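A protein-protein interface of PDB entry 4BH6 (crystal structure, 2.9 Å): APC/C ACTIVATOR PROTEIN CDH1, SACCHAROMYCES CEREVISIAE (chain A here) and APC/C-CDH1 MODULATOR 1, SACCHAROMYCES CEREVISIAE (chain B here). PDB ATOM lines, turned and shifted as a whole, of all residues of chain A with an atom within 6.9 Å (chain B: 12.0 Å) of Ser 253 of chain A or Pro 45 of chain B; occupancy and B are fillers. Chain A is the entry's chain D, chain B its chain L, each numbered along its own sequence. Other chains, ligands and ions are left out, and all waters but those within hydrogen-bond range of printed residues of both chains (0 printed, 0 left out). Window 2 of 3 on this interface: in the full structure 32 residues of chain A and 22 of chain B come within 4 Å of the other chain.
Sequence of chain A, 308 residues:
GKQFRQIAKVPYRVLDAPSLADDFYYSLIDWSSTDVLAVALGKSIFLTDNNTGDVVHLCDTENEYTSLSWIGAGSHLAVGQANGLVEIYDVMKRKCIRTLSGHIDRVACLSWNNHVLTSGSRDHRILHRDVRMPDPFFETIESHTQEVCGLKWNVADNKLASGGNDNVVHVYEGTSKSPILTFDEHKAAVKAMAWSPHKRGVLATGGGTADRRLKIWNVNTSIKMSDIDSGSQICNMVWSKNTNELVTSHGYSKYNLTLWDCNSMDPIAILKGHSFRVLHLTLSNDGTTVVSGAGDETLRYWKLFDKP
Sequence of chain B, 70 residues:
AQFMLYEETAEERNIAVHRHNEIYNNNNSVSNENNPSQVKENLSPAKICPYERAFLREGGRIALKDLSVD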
ATOM      1  N   THR A 209       3.682   1.826 -15.959  1.00  0.00           N
ATOM      2  CA  THR A 209       2.733   1.129 -16.831  1.00  0.00           C
ATOM      3  C   THR A 209       3.096   1.140 -18.301  1.00  0.00           C
ATOM      4  O   THR A 209       3.141   0.085 -18.929  1.00  0.00           O
ATOM      5  CB  THR A 209       1.299   1.653 -16.646  1.00  0.00           C
ATOM      6  OG1 THR A 209       0.918   1.500 -15.267  1.00  0.00           O
ATOM      7  CG2 THR A 209       0.308   0.902 -17.553  1.00  0.00           C
ATOM      8  N   ARG A 212       7.457  -0.621 -18.278  1.00  0.00           N
ATOM      9  CA  ARG A 212       7.516  -2.002 -17.796  1.00  0.00           C
ATOM     10  C   ARG A 212       8.879  -2.617 -17.811  1.00  0.00           C
ATOM     11  O   ARG A 212       9.012  -3.803 -17.489  1.00  0.00           O
ATOM     12  CB  ARG A 212       6.513  -2.893 -18.549  1.00  0.00           C
ATOM     13  CG  ARG A 212       5.062  -2.484 -18.271  1.00  0.00           C
ATOM     14  CD  ARG A 212       4.084  -3.212 -19.149  1.00  0.00           C
ATOM     15  NE  ARG A 212       4.203  -2.789 -20.535  1.00  0.00           N
ATOM     16  CZ  ARG A 212       4.372  -3.620 -21.560  1.00  0.00           C
ATOM     17  NH1 ARG A 212       4.440  -4.952 -21.373  1.00  0.00           N
ATOM     18  NH2 ARG A 212       4.458  -3.113 -22.787  1.00  0.00           N
ATOM     19  N   GLY A 231       7.072  -7.045 -18.586  1.00  0.00           N
ATOM     20  CA  GLY A 231       5.661  -7.278 -18.936  1.00  0.00           C
ATOM     21  C   GLY A 231       4.575  -6.772 -18.001  1.00  0.00           C
ATOM     22  O   GLY A 231       3.420  -7.146 -18.158  1.00  0.00           O
ATOM     23  N   SER A 232       4.929  -5.945 -17.024  1.00  0.00           N
ATOM     24  CA  SER A 232       3.934  -5.275 -16.168  1.00  0.00           C
ATOM     25  C   SER A 232       4.545  -4.069 -15.471  1.00  0.00           C
ATOM     26  O   SER A 232       5.780  -3.947 -15.377  1.00  0.00           O
ATOM     27  CB  SER A 232       3.313  -6.237 -15.142  1.00  0.00           C
ATOM     28  OG  SER A 232       4.266  -6.773 -14.242  1.00  0.00           O
ATOM     29  N   GLN A 233       3.696  -3.181 -14.985  1.00  0.00           N
ATOM     30  CA  GLN A 233       4.154  -1.986 -14.292  1.00  0.00           C
ATOM     31  C   GLN A 233       5.082  -2.342 -13.113  1.00  0.00           C
ATOM     32  O   GLN A 233       4.689  -3.126 -12.236  1.00  0.00           O
ATOM     33  CB  GLN A 233       2.922  -1.228 -13.815  1.00  0.00           C
ATOM     34  CG  GLN A 233       3.178   0.059 -13.072  1.00  0.00           C
ATOM     35  CD  GLN A 233       1.908   0.587 -12.429  1.00  0.00           C
ATOM     36  OE1 GLN A 233       1.114  -0.181 -11.872  1.00  0.00           O
ATOM     37  NE2 GLN A 233       1.707   1.903 -12.500  1.00  0.00           N
ATOM     38  N   HIS A 250       5.072  -5.797  -8.717  1.00  0.00           N
ATOM     39  CA  HIS A 250       4.385  -5.372  -9.934  1.00  0.00           C
ATOM     40  C   HIS A 250       2.961  -4.853  -9.767  1.00  0.00           C
ATOM     41  O   HIS A 250       2.219  -5.257  -8.860  1.00  0.00           O
ATOM     42  CB  HIS A 250       4.467  -6.464 -11.012  1.00  0.00           C
ATOM     43  CG  HIS A 250       5.866  -6.743 -11.456  1.00  0.00           C
ATOM     44  ND1 HIS A 250       6.415  -6.195 -12.597  1.00  0.00           N
ATOM     45  CD2 HIS A 250       6.852  -7.467 -10.877  1.00  0.00           C
ATOM     46  CE1 HIS A 250       7.675  -6.583 -12.708  1.00  0.00           C
ATOM     47  NE2 HIS A 250       7.964  -7.359 -11.678  1.00  0.00           N
ATOM     48  N   GLY A 251       2.615  -3.922 -10.655  1.00  0.00           N
ATOM     49  CA  GLY A 251       1.302  -3.316 -10.699  1.00  0.00           C
ATOM     50  C   GLY A 251       0.570  -3.854 -11.911  1.00  0.00           C
ATOM     51  O   GLY A 251       0.547  -5.067 -12.150  1.00  0.00           O
ATOM     52  N   TYR A 252      -0.020  -2.952 -12.687  1.00  0.00           N
ATOM     53  CA  TYR A 252      -0.824  -3.340 -13.840  1.00  0.00           C
ATOM     54  C   TYR A 252       0.018  -4.138 -14.856  1.00  0.00           C
ATOM     55  O   TYR A 252       1.104  -3.692 -15.223  1.00  0.00           O
ATOM     56  CB  TYR A 252      -1.398  -2.083 -14.514  1.00  0.00           C
ATOM     57  CG  TYR A 252      -2.180  -1.126 -13.624  1.00  0.00           C
ATOM     58  CD1 TYR A 252      -3.325  -1.538 -12.937  1.00  0.00           C
ATOM     59  CD2 TYR A 252      -1.796   0.203 -13.501  1.00  0.00           C
ATOM     60  CE1 TYR A 252      -4.052  -0.660 -12.144  1.00  0.00           C
ATOM     61  CE2 TYR A 252      -2.522   1.090 -12.712  1.00  0.00           C
ATOM     62  CZ  TYR A 252      -3.652   0.648 -12.043  1.00  0.00           C
ATOM     63  OH  TYR A 252      -4.383   1.502 -11.259  1.00  0.00           O
ATOM     64  N   SER A 253      -0.437  -5.308 -15.306  1.00  0.00           N
ATOM     65  CA  SER A 253      -1.659  -5.957 -14.835  1.00  0.00           C
ATOM     66  C   SER A 253      -1.315  -7.338 -14.266  1.00  0.00           C
ATOM     67  O   SER A 253      -2.032  -8.316 -14.518  1.00  0.00           O
ATOM     68  CB  SER A 253      -2.682  -6.112 -15.977  1.00  0.00           C
ATOM     69  OG  SER A 253      -3.071  -4.873 -16.548  1.00  0.00           O
ATOM     70  N   LYS A 254      -0.203  -7.411 -13.527  1.00  0.00           N
ATOM     71  CA  LYS A 254       0.251  -8.652 -12.886  1.00  0.00           C
ATOM     72  C   LYS A 254       0.737  -8.375 -11.459  1.00  0.00           C
ATOM     73  O   LYS A 254       1.909  -8.036 -11.266  1.00  0.00           O
ATOM     74  CB  LYS A 254       1.401  -9.282 -13.671  1.00  0.00           C
ATOM     75  CG  LYS A 254       1.112  -9.628 -15.116  1.00  0.00           C
ATOM     76  CD  LYS A 254       0.580 -11.044 -15.260  1.00  0.00           C
ATOM     77  CE  LYS A 254       0.128 -11.308 -16.684  1.00  0.00           C
ATOM     78  NZ  LYS A 254       1.247 -11.015 -17.622  1.00  0.00           N
ATOM     79  N   TYR A 255      -0.141  -8.545 -10.471  1.00  0.00           N
ATOM     80  CA  TYR A 255       0.174  -8.233  -9.078  1.00  0.00           C
ATOM     81  C   TYR A 255       1.076  -9.282  -8.406  1.00  0.00           C
ATOM     82  O   TYR A 255       0.695  -9.934  -7.423  1.00  0.00           O
ATOM     83  CB  TYR A 255      -1.111  -8.001  -8.280  1.00  0.00           C
ATOM     84  CG  TYR A 255      -2.064  -7.022  -8.926  1.00  0.00           C
ATOM     85  CD1 TYR A 255      -1.611  -6.101  -9.888  1.00  0.00           C
ATOM     86  CD2 TYR A 255      -3.405  -6.983  -8.561  1.00  0.00           C
ATOM     87  CE1 TYR A 255      -2.476  -5.184 -10.479  1.00  0.00           C
ATOM     88  CE2 TYR A 255      -4.276  -6.069  -9.146  1.00  0.00           C
ATOM     89  CZ  TYR A 255      -3.807  -5.178 -10.101  1.00  0.00           C
ATOM     90  OH  TYR A 255      -4.666  -4.284 -10.686  1.00  0.00           O
ATOM     91  N   ASN A 256       2.289  -9.417  -8.944  1.00  0.00           N
ATOM     92  CA  ASN A 256       3.287 -10.375  -8.450  1.00  0.00           C
ATOM     93  C   ASN A 256       4.565  -9.721  -7.928  1.00  0.00           C
ATOM     94  O   ASN A 256       4.820  -8.520  -8.166  1.00  0.00           O
ATOM     95  CB  ASN A 256       3.697 -11.315  -9.569  1.00  0.00           C
ATOM     96  CG  ASN A 256       2.523 -11.917 -10.284  1.00  0.00           C
ATOM     97  OD1 ASN A 256       2.531 -12.056 -11.513  1.00  0.00           O
ATOM     98  ND2 ASN A 256       1.497 -12.280  -9.522  1.00  0.00           N
ATOM     99  N   VAL B  39      -0.750  11.817 -12.156  1.00  0.00           N
ATOM    100  CA  VAL B  39      -1.419  10.721 -11.509  1.00  0.00           C
ATOM    101  C   VAL B  39      -1.455   9.514 -12.466  1.00  0.00           C
ATOM    102  O   VAL B  39      -2.177   8.560 -12.244  1.00  0.00           O
ATOM    103  CB  VAL B  39      -2.821  11.200 -11.034  1.00  0.00           C
ATOM    104  CG1 VAL B  39      -3.867  11.177 -12.161  1.00  0.00           C
ATOM    105  CG2 VAL B  39      -3.291  10.399  -9.834  1.00  0.00           C
ATOM    106  N   LYS B  40      -0.642   9.551 -13.518  1.00  0.00           N
ATOM    107  CA  LYS B  40      -0.663   8.526 -14.590  1.00  0.00           C
ATOM    108  C   LYS B  40      -0.428   7.090 -14.140  1.00  0.00           C
ATOM    109  O   LYS B  40      -0.958   6.165 -14.730  1.00  0.00           O
ATOM    110  CB  LYS B  40       0.359   8.868 -15.689  1.00  0.00           C
ATOM    111  CG  LYS B  40       1.813   8.788 -15.257  1.00  0.00           C
ATOM    112  CD  LYS B  40       2.735   9.152 -16.394  1.00  0.00           C
ATOM    113  CE  LYS B  40       4.132   9.292 -15.833  1.00  0.00           C
ATOM    114  NZ  LYS B  40       5.155   9.715 -16.821  1.00  0.00           N
ATOM    115  N   GLU B  41       0.396   6.894 -13.114  1.00  0.00           N
ATOM    116  CA  GLU B  41       0.718   5.541 -12.708  1.00  0.00           C
ATOM    117  C   GLU B  41      -0.386   4.939 -11.853  1.00  0.00           C
ATOM    118  O   GLU B  41      -0.267   3.810 -11.409  1.00  0.00           O
ATOM    119  CB  GLU B  41       2.059   5.510 -12.003  1.00  0.00           C
ATOM    120  CG  GLU B  41       3.180   5.932 -12.920  1.00  0.00           C
ATOM    121  CD  GLU B  41       3.459   4.942 -14.058  1.00  0.00           C
ATOM    122  OE1 GLU B  41       3.303   3.703 -13.847  1.00  0.00           O
ATOM    123  OE2 GLU B  41       3.871   5.393 -15.167  1.00  0.00           O
ATOM    124  N   ASN B  42      -1.459   5.688 -11.627  1.00  0.00           N
ATOM    125  CA  ASN B  42      -2.591   5.192 -10.855  1.00  0.00           C
ATOM    126  C   ASN B  42      -3.845   4.896 -11.683  1.00  0.00           C
ATOM    127  O   ASN B  42      -4.887   4.508 -11.134  1.00  0.00           O
ATOM    128  CB  ASN B  42      -2.952   6.191  -9.791  1.00  0.00           C
ATOM    129  CG  ASN B  42      -2.095   6.068  -8.578  1.00  0.00           C
ATOM    130  OD1 ASN B  42      -1.862   7.016  -7.897  1.00  0.00           O
ATOM    131  ND2 ASN B  42      -1.646   4.916  -8.296  1.00  0.00           N
ATOM    132  N   LEU B  43      -3.735   5.126 -12.988  1.00  0.00           N
ATOM    133  CA  LEU B  43      -4.750   4.776 -13.976  1.00  0.00           C
ATOM    134  C   LEU B  43      -4.501   3.372 -14.513  1.00  0.00           C
ATOM    135  O   LEU B  43      -3.495   3.130 -15.177  1.00  0.00           O
ATOM    136  CB  LEU B  43      -4.725   5.754 -15.150  1.00  0.00           C
ATOM    137  CG  LEU B  43      -4.853   7.228 -14.778  1.00  0.00           C
ATOM    138  CD1 LEU B  43      -4.437   8.062 -15.971  1.00  0.00           C
ATOM    139  CD2 LEU B  43      -6.251   7.616 -14.330  1.00  0.00           C
ATOM    140  N   SEP B  44      -5.429   2.455 -14.219  1.00  0.00           N
ATOM    141  CA  SEP B  44      -5.394   1.085 -14.713  1.00  0.00           C
ATOM    142  CB  SEP B  44      -6.498   0.407 -13.967  1.00  0.00           C
ATOM    143  OG  SEP B  44      -7.729   1.006 -14.347  1.00  0.00           O
ATOM    144  C   SEP B  44      -5.659   1.079 -16.191  1.00  0.00           C
ATOM    145  O   SEP B  44      -6.201   2.029 -16.727  1.00  0.00           O
ATOM    146  P   SEP B  44      -9.102   0.566 -13.596  1.00  0.00           P
ATOM    147  O1P SEP B  44      -8.830   0.875 -12.119  1.00  0.00           O
ATOM    148  O2P SEP B  44     -10.196   1.372 -14.254  1.00  0.00           O
ATOM    149  O3P SEP B  44      -9.219  -0.902 -13.938  1.00  0.00           O
ATOM    150  N   PRO B  45      -5.268   0.014 -16.898  1.00  0.00           N
ATOM    151  CA  PRO B  45      -5.382   0.043 -18.364  1.00  0.00           C
ATOM    152  C   PRO B  45      -6.819   0.155 -18.872  1.00  0.00           C
ATOM    153  O   PRO B  45      -7.032   0.619 -19.983  1.00  0.00           O
ATOM    154  CB  PRO B  45      -4.755  -1.285 -18.814  1.00  0.00           C
ATOM    155  CG  PRO B  45      -3.975  -1.769 -17.658  1.00  0.00           C
ATOM    156  CD  PRO B  45      -4.668  -1.243 -16.427  1.00  0.00           C
ATOM    157  N   ALA B  46      -7.798  -0.252 -18.075  1.00  0.00           N
ATOM    158  CA  ALA B  46      -9.191   0.014 -18.431  1.00  0.00           C
ATOM    159  C   ALA B  46      -9.425   1.511 -18.638  1.00  0.00           C
ATOM    160  O   ALA B  46     -10.074   1.899 -19.614  1.00  0.00           O
ATOM    161  CB  ALA B  46     -10.144  -0.525 -17.378  1.00  0.00           C
ATOM    162  N   LYS B  47      -8.897   2.335 -17.716  1.00  0.00           N
ATOM    163  CA  LYS B  47      -8.938   3.800 -17.836  1.00  0.00           C
ATOM    164  C   LYS B  47      -8.030   4.351 -18.939  1.00  0.00           C
ATOM    165  O   LYS B  47      -8.454   5.271 -19.632  1.00  0.00           O
ATOM    166  CB  LYS B  47      -8.631   4.516 -16.513  1.00  0.00           C
ATOM    167  CG  LYS B  47      -9.629   4.269 -15.413  1.00  0.00           C
ATOM    168  CD  LYS B  47      -9.483   5.282 -14.322  1.00  0.00           C
ATOM    169  CE  LYS B  47     -10.542   4.998 -13.293  1.00  0.00           C
ATOM    170  NZ  LYS B  47     -10.148   3.702 -12.685  1.00  0.00           N
ATOM    171  N   ILE B  48      -6.803   3.826 -19.101  1.00  0.00           N
ATOM    172  CA  ILE B  48      -5.960   4.237 -20.240  1.00  0.00           C
ATOM    173  C   ILE B  48      -6.624   3.880 -21.583  1.00  0.00           C
ATOM    174  O   ILE B  48      -6.444   4.608 -22.566  1.00  0.00           O
ATOM    175  CB  ILE B  48      -4.527   3.682 -20.157  1.00  0.00           C
ATOM    176  CG1 ILE B  48      -3.826   4.261 -18.945  1.00  0.00           C
ATOM    177  CG2 ILE B  48      -3.713   4.056 -21.391  1.00  0.00           C
ATOM    178  CD1 ILE B  48      -2.577   3.505 -18.566  1.00  0.00           C
ATOM    179  N   CYS B  49      -7.393   2.776 -21.598  1.00  0.00           N
ATOM    180  CA  CYS B  49      -8.290   2.379 -22.720  1.00  0.00           C
ATOM    181  C   CYS B  49      -7.522   2.488 -24.046  1.00  0.00           C
ATOM    182  O   CYS B  49      -8.083   2.913 -25.042  1.00  0.00           O
ATOM    183  CB  CYS B  49      -9.509   3.324 -22.761  1.00  0.00           C
ATOM    184  SG  CYS B  49     -11.150   2.585 -22.670  1.00  0.00           S
ATOM    185  N   PRO B  50      -6.262   2.025 -24.067  1.00  0.00           N
ATOM    186  CA  PRO B  50      -5.075   2.627 -24.686  1.00  0.00           C
ATOM    187  C   PRO B  50      -4.944   2.774 -26.206  1.00  0.00           C
ATOM    188  O   PRO B  50      -5.229   3.841 -26.720  1.00  0.00           O
ATOM    189  CB  PRO B  50      -3.927   1.779 -24.132  1.00  0.00           C
ATOM    190  CG  PRO B  50      -4.552   0.473 -23.741  1.00  0.00           C
ATOM    191  CD  PRO B  50      -6.050   0.600 -23.777  1.00  0.00           C
ATOM    192  N   TYR B  51      -4.459   1.753 -26.912  1.00  0.00           N
ATOM    193  CA  TYR B  51      -4.016   1.949 -28.298  1.00  0.00           C
ATOM    194  C   TYR B  51      -4.829   1.339 -29.455  1.00  0.00           C
ATOM    195  O   TYR B  51      -5.488   2.085 -30.124  1.00  0.00           O
ATOM    196  CB  TYR B  51      -2.510   1.728 -28.441  1.00  0.00           C
ATOM    197  CG  TYR B  51      -1.702   2.876 -27.875  1.00  0.00           C
ATOM    198  CD1 TYR B  51      -1.478   4.036 -28.631  1.00  0.00           C
ATOM    199  CD2 TYR B  51      -1.175   2.811 -26.579  1.00  0.00           C
ATOM    200  CE1 TYR B  51      -0.740   5.092 -28.120  1.00  0.00           C
ATOM    201  CE2 TYR B  51      -0.435   3.861 -26.054  1.00  0.00           C
ATOM    202  CZ  TYR B  51      -0.219   5.003 -26.833  1.00  0.00           C
ATOM    203  OH  TYR B  51       0.512   6.065 -26.334  1.00  0.00           O
ATOM    204  N   GLU B  52      -4.762   0.052 -29.785  1.00  0.00           N
ATOM    205  CA  GLU B  52      -5.645  -0.514 -30.883  1.00  0.00           C
ATOM    206  C   GLU B  52      -7.154  -0.169 -30.632  1.00  0.00           C
ATOM    207  O   GLU B  52      -7.497   0.132 -29.494  1.00  0.00           O
ATOM    208  CB  GLU B  52      -5.405  -2.028 -31.033  1.00  0.00           C
ATOM    209  CG  GLU B  52      -5.035  -2.710 -29.716  1.00  0.00           C
ATOM    210  CD  GLU B  52      -5.688  -2.024 -28.522  1.00  0.00           C
ATOM    211  OE1 GLU B  52      -6.852  -2.336 -28.225  1.00  0.00           O
ATOM    212  OE2 GLU B  52      -5.059  -1.131 -27.913  1.00  0.00           O
ATOM    213  N   ARG B  53      -8.090  -0.244 -31.587  1.00  0.00           N
ATOM    214  CA  ARG B  53      -8.186  -1.149 -32.746  1.00  0.00           C
ATOM    215  C   ARG B  53      -7.088  -1.124 -33.824  1.00  0.00           C
ATOM    216  O   ARG B  53      -7.126  -1.914 -34.794  1.00  0.00           O
ATOM    217  CB  ARG B  53      -9.574  -0.982 -33.402  1.00  0.00           C
ATOM    218  CG  ARG B  53     -10.130   0.448 -33.438  1.00  0.00           C
ATOM    219  CD  ARG B  53      -9.274   1.449 -34.226  1.00  0.00           C
ATOM    220  NE  ARG B  53     -10.044   2.541 -34.841  1.00  0.00           N
ATOM    221  CZ  ARG B  53     -10.286   2.653 -36.151  1.00  0.00           C
ATOM    222  NH1 ARG B  53      -9.809   1.752 -36.997  1.00  0.00           N
ATOM    223  NH2 ARG B  53     -10.998   3.669 -36.629  1.00  0.00           N
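The backbone carbonyl oxygen (O) of Thr 209 of chain A sits close to the guanidinium group (NE) of Arg 212 of chain A. The side-chain hydroxyl of Thr 209 of chain A is in hydrogen-bond range of the side-chain amide nitrogen of Gln 233 of chain A, at 2.9 Å. The backbone carbonyl oxygen of Gln 233 of chain A sits at hydrogen-bond distance from the backbone NH of Gly 251 of chain A, 2.7 Å away. O of Tyr 252 of chain A is in hydrogen-bond range of N of Gln 233 of chain A. O2P of SEP 44 of chain B sits close to NZ of Lys 47 of chain B (2.8 Å).
Tyr 252 of chain A touches Glu 41 of chain B (CE2 to O, 3.8 Å). Tyr 252 of chain A touches Leu 43 of chain B (CE2 to O, 3.3 Å). Tyr 252 of chain A touches Pro 45 of chain B (CG to CD, 3.7 Å). CG of Pro 45 of chain B touches OG of Ser 253 of chain A (3.4 Å).
Of the printed residues of chain B, Thr 209 of chain A touches Glu 41. No residue of chain B comes within 4 Å of Ser 232 of chain A. Of the printed residues of chain B, Gln 233 of chain A touches Glu 41 (2.8 Å). Gly 251 of chain A touches none of the printed residues of chain B. Tyr 252 of chain A touches just these residues of chain B: Glu 41 (3.8 Å), Asn 42 (3.1 Å), Leu 43 (3.3 Å), SEP 44 (3.2 Å) and Pro 45 (3.7 Å). No residue of chain B comes within 4 Å of Tyr 255 of chain A. Of the printed residues of chain A, Glu 41 of chain B touches Thr 209 (2.9 Å), Gln 233 (2.8 Å) and Tyr 252 (3.8 Å). Of the printed residues of chain A, Leu 43 of chain B touches Tyr 252. Of the printed residues of chain A, SEP 44 of chain B touches Tyr 252. Of chain A, only Tyr 252 and Ser 253 come within 4 Å of Pro 45 of chain B. The nearest residue of chain B that does not touch Ser 253 of chain A is SEP 44 of chain B (6.5 Å).
The backbone NH (N) of Thr 209 of chain A sits at hydrogen-bond distance from the side-chain carboxylate (OE1) of Glu 41 of chain B. NE2 of Gln 233 of chain A sits at hydrogen-bond distance from OE1 of Glu 41 of chain B (2.8 Å). The backbone carbonyl oxygen of Asn 42 of chain B lies within hydrogen-bond range of the side-chain hydroxyl of Tyr 252 of chain A. The side-chain hydroxyl of Tyr 252 of chain A lies within hydrogen-bond range of N of SEP 44 of chain B, 3.3 Å away.
Of the 12 printed residues of chain A, 4 touch a printed residue of chain B. Hydrophobic or aromatic side chains of chain A that line the printed part of chain B: Tyr 252. Printed residues of chain B that touch a printed residue of chain A: Glu 41, Asn 42, Leu 43, SEP 44 and Pro 45. Hydrophobic or aromatic side chains of chain B within 4 Å of the printed part of chain A: Pro 45. Among the printed residues, no Asp or Glu carboxylate lies within 4 Å of a Lys or Arg side-chain nitrogen of the other chain.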
